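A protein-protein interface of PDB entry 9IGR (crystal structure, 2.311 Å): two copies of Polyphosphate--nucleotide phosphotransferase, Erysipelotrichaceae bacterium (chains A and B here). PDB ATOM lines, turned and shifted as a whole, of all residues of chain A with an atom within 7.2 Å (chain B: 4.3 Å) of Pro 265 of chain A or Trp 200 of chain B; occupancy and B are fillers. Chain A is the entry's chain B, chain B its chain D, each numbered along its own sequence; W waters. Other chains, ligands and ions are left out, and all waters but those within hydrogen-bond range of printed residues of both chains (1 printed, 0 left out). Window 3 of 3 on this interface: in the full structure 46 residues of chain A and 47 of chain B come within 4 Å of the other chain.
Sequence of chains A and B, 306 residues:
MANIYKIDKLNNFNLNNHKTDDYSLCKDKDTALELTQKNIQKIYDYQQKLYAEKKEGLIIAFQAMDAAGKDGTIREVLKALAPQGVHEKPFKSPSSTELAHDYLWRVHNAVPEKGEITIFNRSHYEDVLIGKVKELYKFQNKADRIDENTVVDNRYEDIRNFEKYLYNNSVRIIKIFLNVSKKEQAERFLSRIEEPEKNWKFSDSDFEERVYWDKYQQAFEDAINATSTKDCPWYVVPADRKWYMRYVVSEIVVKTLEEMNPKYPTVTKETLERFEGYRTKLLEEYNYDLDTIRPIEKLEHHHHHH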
ATOM      1  N   GLN A  48      19.888   1.921   9.369  1.00  0.00           N
ATOM      2  CA  GLN A  48      21.332   1.699   9.279  1.00  0.00           C
ATOM      3  C   GLN A  48      21.629   0.414   8.507  1.00  0.00           C
ATOM      4  O   GLN A  48      22.536   0.348   7.705  1.00  0.00           O
ATOM      5  CB  GLN A  48      21.975   1.581  10.655  1.00  0.00           C
ATOM      6  CG  GLN A  48      21.626   2.728  11.599  1.00  0.00           C
ATOM      7  CD  GLN A  48      21.929   4.050  10.932  1.00  0.00           C
ATOM      8  OE1 GLN A  48      23.084   4.284  10.574  1.00  0.00           O
ATOM      9  NE2 GLN A  48      20.921   4.902  10.749  1.00  0.00           N
ATOM     10  N   LYS A  49      20.848  -0.637   8.736  1.00  0.00           N
ATOM     11  CA  LYS A  49      21.057  -1.853   7.974  1.00  0.00           C
ATOM     12  C   LYS A  49      20.670  -1.645   6.511  1.00  0.00           C
ATOM     13  O   LYS A  49      21.364  -2.099   5.672  1.00  0.00           O
ATOM     14  CB  LYS A  49      20.326  -3.017   8.591  1.00  0.00           C
ATOM     15  CG  LYS A  49      20.713  -3.296  10.007  1.00  0.00           C
ATOM     16  CD  LYS A  49      19.693  -4.182  10.725  1.00  0.00           C
ATOM     17  CE  LYS A  49      20.257  -4.486  12.069  1.00  0.00           C
ATOM     18  NZ  LYS A  49      19.260  -5.351  12.689  1.00  0.00           N
ATOM     19  N   TYR A  51      20.850   1.117   4.683  1.00  0.00           N
ATOM     20  CA  TYR A  51      21.915   1.903   4.082  1.00  0.00           C
ATOM     21  C   TYR A  51      23.164   1.049   3.831  1.00  0.00           C
ATOM     22  O   TYR A  51      23.883   1.232   2.868  1.00  0.00           O
ATOM     23  CB  TYR A  51      22.274   3.093   4.991  1.00  0.00           C
ATOM     24  CG  TYR A  51      23.202   4.103   4.347  1.00  0.00           C
ATOM     25  CD1 TYR A  51      22.761   4.889   3.276  1.00  0.00           C
ATOM     26  CD2 TYR A  51      24.479   4.318   4.848  1.00  0.00           C
ATOM     27  CE1 TYR A  51      23.599   5.814   2.676  1.00  0.00           C
ATOM     28  CE2 TYR A  51      25.314   5.259   4.283  1.00  0.00           C
ATOM     29  CZ  TYR A  51      24.875   5.980   3.182  1.00  0.00           C
ATOM     30  OH  TYR A  51      25.703   6.905   2.648  1.00  0.00           O
ATOM     31  N   ALA A  52      23.494   0.152   4.745  1.00  0.00           N
ATOM     32  CA  ALA A  52      24.701  -0.621   4.586  1.00  0.00           C
ATOM     33  C   ALA A  52      24.549  -1.640   3.449  1.00  0.00           C
ATOM     34  O   ALA A  52      25.507  -1.959   2.777  1.00  0.00           O
ATOM     35  CB  ALA A  52      25.043  -1.316   5.871  1.00  0.00           C
ATOM     36  N   GLU A  53      23.364  -2.173   3.254  1.00  0.00           N
ATOM     37  CA  GLU A  53      23.128  -3.245   2.307  1.00  0.00           C
ATOM     38  C   GLU A  53      23.001  -2.747   0.870  1.00  0.00           C
ATOM     39  O   GLU A  53      23.279  -3.504  -0.037  1.00  0.00           O
ATOM     40  CB  GLU A  53      21.927  -4.046   2.777  1.00  0.00           C
ATOM     41  CG  GLU A  53      22.077  -5.512   2.370  1.00  0.00           C
ATOM     42  CD  GLU A  53      21.006  -6.475   2.818  1.00  0.00           C
ATOM     43  OE1 GLU A  53      19.873  -5.984   3.102  1.00  0.00           O
ATOM     44  OE2 GLU A  53      21.392  -7.680   2.870  1.00  0.00           O
ATOM     45  N   LYS A  54      22.553  -1.508   0.638  1.00  0.00           N
ATOM     46  CA  LYS A  54      22.444  -0.957  -0.710  1.00  0.00           C
ATOM     47  C   LYS A  54      21.686  -1.901  -1.643  1.00  0.00           C
ATOM     48  O   LYS A  54      22.049  -2.004  -2.794  1.00  0.00           O
ATOM     49  CB  LYS A  54      23.884  -0.652  -1.184  1.00  0.00           C
ATOM     50  CG  LYS A  54      24.270   0.682  -0.487  1.00  0.00           C
ATOM     51  CD  LYS A  54      25.702   1.130  -0.583  1.00  0.00           C
ATOM     52  CE  LYS A  54      26.215   1.772   0.705  1.00  0.00           C
ATOM     53  NZ  LYS A  54      25.424   2.912   1.168  1.00  0.00           N
ATOM     54  N   LYS A  55      20.596  -2.530  -1.176  1.00  0.00           N
ATOM     55  CA  LYS A  55      19.771  -3.396  -2.014  1.00  0.00           C
ATOM     56  C   LYS A  55      18.355  -2.934  -2.335  1.00  0.00           C
ATOM     57  O   LYS A  55      17.782  -3.465  -3.283  1.00  0.00           O
ATOM     58  CB  LYS A  55      19.560  -4.701  -1.250  1.00  0.00           C
ATOM     59  CG  LYS A  55      20.728  -5.642  -1.466  1.00  0.00           C
ATOM     60  CD  LYS A  55      20.378  -7.003  -0.889  1.00  0.00           C
ATOM     61  CE  LYS A  55      21.617  -7.869  -0.947  1.00  0.00           C
ATOM     62  NZ  LYS A  55      21.132  -8.960  -0.112  1.00  0.00           N
ATOM     63  N   LYS A 263      19.926  -6.396   6.299  1.00  0.00           N
ATOM     64  CA  LYS A 263      21.006  -7.012   7.054  1.00  0.00           C
ATOM     65  C   LYS A 263      22.316  -6.319   6.711  1.00  0.00           C
ATOM     66  O   LYS A 263      22.514  -5.881   5.613  1.00  0.00           O
ATOM     67  CB  LYS A 263      21.071  -8.506   6.705  1.00  0.00           C
ATOM     68  CG  LYS A 263      19.992  -9.205   7.547  1.00  0.00           C
ATOM     69  CD  LYS A 263      19.573 -10.605   7.174  1.00  0.00           C
ATOM     70  CE  LYS A 263      19.025 -10.667   5.768  1.00  0.00           C
ATOM     71  NZ  LYS A 263      18.684 -12.078   5.537  1.00  0.00           N
ATOM     72  N   TYR A 264      23.207  -6.179   7.658  1.00  0.00           N
ATOM     73  CA  TYR A 264      24.562  -5.765   7.364  1.00  0.00           C
ATOM     74  C   TYR A 264      25.116  -6.841   6.453  1.00  0.00           C
ATOM     75  O   TYR A 264      24.863  -8.014   6.677  1.00  0.00           O
ATOM     76  CB  TYR A 264      25.352  -5.664   8.669  1.00  0.00           C
ATOM     77  CG  TYR A 264      24.936  -4.488   9.538  1.00  0.00           C
ATOM     78  CD1 TYR A 264      25.157  -3.182   9.113  1.00  0.00           C
ATOM     79  CD2 TYR A 264      24.325  -4.676  10.766  1.00  0.00           C
ATOM     80  CE1 TYR A 264      24.741  -2.086   9.867  1.00  0.00           C
ATOM     81  CE2 TYR A 264      23.948  -3.583  11.553  1.00  0.00           C
ATOM     82  CZ  TYR A 264      24.163  -2.293  11.104  1.00  0.00           C
ATOM     83  OH  TYR A 264      23.795  -1.163  11.803  1.00  0.00           O
ATOM     84  N   PRO A 265      25.788  -6.493   5.341  1.00  0.00           N
ATOM     85  CA  PRO A 265      26.316  -7.511   4.428  1.00  0.00           C
ATOM     86  C   PRO A 265      27.472  -8.287   5.031  1.00  0.00           C
ATOM     87  O   PRO A 265      28.219  -7.730   5.788  1.00  0.00           O
ATOM     88  CB  PRO A 265      26.907  -6.758   3.213  1.00  0.00           C
ATOM     89  CG  PRO A 265      26.545  -5.288   3.483  1.00  0.00           C
ATOM     90  CD  PRO A 265      26.101  -5.122   4.919  1.00  0.00           C
ATOM     91  N   THR A 266      27.604  -9.556   4.707  1.00  0.00           N
ATOM     92  CA  THR A 266      28.677 -10.387   5.183  1.00  0.00           C
ATOM     93  C   THR A 266      29.620 -10.382   3.987  1.00  0.00           C
ATOM     94  O   THR A 266      29.152 -10.424   2.844  1.00  0.00           O
ATOM     95  CB  THR A 266      28.205 -11.805   5.593  1.00  0.00           C
ATOM     96  OG1 THR A 266      27.890 -12.405   4.357  1.00  0.00           O
ATOM     97  CG2 THR A 266      26.878 -11.874   6.344  1.00  0.00           C
ATOM     98  N   VAL A 267      30.932 -10.316   4.229  1.00  0.00           N
ATOM     99  CA  VAL A 267      31.822 -10.235   3.080  1.00  0.00           C
ATOM    100  C   VAL A 267      32.184 -11.646   2.589  1.00  0.00           C
ATOM    101  O   VAL A 267      32.050 -12.625   3.311  1.00  0.00           O
ATOM    102  CB  VAL A 267      33.043  -9.366   3.406  1.00  0.00           C
ATOM    103  CG1 VAL A 267      32.648  -7.898   3.554  1.00  0.00           C
ATOM    104  CG2 VAL A 267      33.797  -9.914   4.608  1.00  0.00           C
ATOM    105  N   PHE A 275      41.347  -9.341   4.448  1.00  0.00           N
ATOM    106  CA  PHE A 275      41.140  -8.571   5.663  1.00  0.00           C
ATOM    107  C   PHE A 275      42.033  -9.076   6.797  1.00  0.00           C
ATOM    108  O   PHE A 275      42.601  -8.270   7.517  1.00  0.00           O
ATOM    109  CB  PHE A 275      39.654  -8.551   6.020  1.00  0.00           C
ATOM    110  CG  PHE A 275      38.840  -7.548   5.207  1.00  0.00           C
ATOM    111  CD1 PHE A 275      39.364  -6.936   4.060  1.00  0.00           C
ATOM    112  CD2 PHE A 275      37.521  -7.262   5.533  1.00  0.00           C
ATOM    113  CE1 PHE A 275      38.615  -6.047   3.294  1.00  0.00           C
ATOM    114  CE2 PHE A 275      36.789  -6.332   4.790  1.00  0.00           C
ATOM    115  CZ  PHE A 275      37.325  -5.757   3.658  1.00  0.00           C
ATOM    116  N   GLU B 197      29.464  -6.513  11.723  1.00  0.00           N
ATOM    117  CA  GLU B 197      28.512  -5.488  11.325  1.00  0.00           C
ATOM    118  C   GLU B 197      29.215  -4.266  10.771  1.00  0.00           C
ATOM    119  O   GLU B 197      28.546  -3.354  10.282  1.00  0.00           O
ATOM    120  CB  GLU B 197      27.692  -4.914  12.486  1.00  0.00           C
ATOM    121  CG  GLU B 197      26.910  -5.948  13.311  1.00  0.00           C
ATOM    122  CD  GLU B 197      25.809  -5.370  14.234  1.00  0.00           C
ATOM    123  OE1 GLU B 197      25.795  -4.147  14.659  1.00  0.00           O
ATOM    124  OE2 GLU B 197      24.898  -6.203  14.496  1.00  0.00           O
ATOM    125  N   LYS B 198      30.550  -4.220  10.833  1.00  0.00           N
ATOM    126  CA  LYS B 198      31.260  -3.100  10.238  1.00  0.00           C
ATOM    127  C   LYS B 198      32.151  -3.499   9.040  1.00  0.00           C
ATOM    128  O   LYS B 198      32.822  -2.664   8.450  1.00  0.00           O
ATOM    129  CB  LYS B 198      32.129  -2.476  11.321  1.00  0.00           C
ATOM    130  CG  LYS B 198      31.385  -1.892  12.508  1.00  0.00           C
ATOM    131  CD  LYS B 198      32.422  -1.159  13.349  1.00  0.00           C
ATOM    132  CE  LYS B 198      32.029  -0.501  14.623  1.00  0.00           C
ATOM    133  NZ  LYS B 198      33.237   0.108  15.185  1.00  0.00           N
ATOM    134  N   ASN B 199      32.178  -4.766   8.677  1.00  0.00           N
ATOM    135  CA  ASN B 199      32.968  -5.239   7.547  1.00  0.00           C
ATOM    136  C   ASN B 199      32.672  -4.480   6.260  1.00  0.00           C
ATOM    137  O   ASN B 199      33.567  -4.105   5.529  1.00  0.00           O
ATOM    138  CB  ASN B 199      32.697  -6.708   7.283  1.00  0.00           C
ATOM    139  CG  ASN B 199      33.445  -7.588   8.223  1.00  0.00           C
ATOM    140  OD1 ASN B 199      34.389  -7.161   8.886  1.00  0.00           O
ATOM    141  ND2 ASN B 199      33.156  -8.849   8.112  1.00  0.00           N
ATOM    142  N   TRP B 200      31.409  -4.177   6.030  1.00  0.00           N
ATOM    143  CA  TRP B 200      31.009  -3.521   4.810  1.00  0.00           C
ATOM    144  C   TRP B 200      31.729  -2.200   4.653  1.00  0.00           C
ATOM    145  O   TRP B 200      31.731  -1.649   3.570  1.00  0.00           O
ATOM    146  CB  TRP B 200      29.468  -3.348   4.787  1.00  0.00           C
ATOM    147  CG  TRP B 200      28.919  -2.278   5.696  1.00  0.00           C
ATOM    148  CD1 TRP B 200      28.642  -2.431   7.014  1.00  0.00           C
ATOM    149  CD2 TRP B 200      28.598  -0.902   5.389  1.00  0.00           C
ATOM    150  NE1 TRP B 200      28.156  -1.242   7.529  1.00  0.00           N
ATOM    151  CE2 TRP B 200      28.117  -0.297   6.571  1.00  0.00           C
ATOM    152  CE3 TRP B 200      28.683  -0.105   4.243  1.00  0.00           C
ATOM    153  CZ2 TRP B 200      27.764   1.044   6.650  1.00  0.00           C
ATOM    154  CZ3 TRP B 200      28.359   1.240   4.300  1.00  0.00           C
ATOM    155  CH2 TRP B 200      27.886   1.802   5.497  1.00  0.00           C
ATOM    156  N   LYS B 201      32.237  -1.645   5.740  1.00  0.00           N
ATOM    157  CA  LYS B 201      32.748  -0.272   5.732  1.00  0.00           C
ATOM    158  C   LYS B 201      34.228  -0.239   5.383  1.00  0.00           C
ATOM    159  O   LYS B 201      34.815   0.819   5.308  1.00  0.00           O
ATOM    160  CB  LYS B 201      32.701   0.367   7.125  1.00  0.00           C
ATOM    161  CG  LYS B 201      31.301   0.600   7.607  1.00  0.00           C
ATOM    162  CD  LYS B 201      31.152   1.384   8.898  1.00  0.00           C
ATOM    163  CE  LYS B 201      31.643   2.725   8.713  1.00  0.00           C
ATOM    164  NZ  LYS B 201      31.304   3.384   9.987  1.00  0.00           N
ATOM    165  N   PHE B 202      34.843  -1.412   5.251  1.00  0.00           N
ATOM    166  CA  PHE B 202      36.278  -1.488   5.095  1.00  0.00           C
ATOM    167  C   PHE B 202      36.555  -1.817   3.643  1.00  0.00           C
ATOM    168  O   PHE B 202      35.915  -2.710   3.101  1.00  0.00           O
ATOM    169  CB  PHE B 202      36.853  -2.597   5.989  1.00  0.00           C
ATOM    170  CG  PHE B 202      38.352  -2.482   6.088  1.00  0.00           C
ATOM    171  CD1 PHE B 202      38.931  -1.369   6.676  1.00  0.00           C
ATOM    172  CD2 PHE B 202      39.175  -3.409   5.516  1.00  0.00           C
ATOM    173  CE1 PHE B 202      40.305  -1.196   6.672  1.00  0.00           C
ATOM    174  CE2 PHE B 202      40.531  -3.236   5.535  1.00  0.00           C
ATOM    175  CZ  PHE B 202      41.095  -2.137   6.107  1.00  0.00           C
HETATM  176  O   HOH W   1      29.146  -5.596   7.225  1.00  0.00           O
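Pro 265 of chain A touches one residue of chain B. Trp 200 of chain B touches just these residues of chain A: Ala 52 (3.3 Å), Tyr 264 (3.9 Å) and Pro 265 (3.7 Å). Printed residues of chain A within 4 Å of Glu 197 of chain B: Tyr 264 (3.6 Å). Of the printed residues of chain A, Phe 202 of chain B touches Phe 275. Lys 54 of chain A touches none of the printed residues of chain B.
Of the 13 printed residues of chain A, 5 touch a printed residue of chain B. Of the 6 printed residues of chain B, 4 touch a printed residue of chain A. Hydrophobic or aromatic side chains of chain B within 4 Å of the printed part of chain A: Trp 200 and Phe 202.
Water W1 lies within hydrogen-bond range of O of Pro 265 of chain A (2.7 Å), N of Trp 200 of chain B (2.9 Å) and N of Asn 199 of chain B (3.5 Å).
Trp 200 of chain B touches Ala 52 of chain A. Glu 197 of chain B touches Tyr 264 of chain A. Trp 200 of chain B touches Tyr 264 of chain A (NE1 to CD1, 3.9 Å). Pro 265 of chain A touches Trp 200 of chain B. CG2 of Val 267 of chain A touches ND2 of Asn 199 of chain B, 3.7 Å away. Asn 199 of chain B touches Phe 275 of chain A (O to CE2, 3.99 Å). Phe 202 of chain B touches Phe 275 of chain A.
O of Glu 197 of chain B sits close to NE1 of Trp 200 of chain B (3.5 Å).
No position is printed for both chains.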
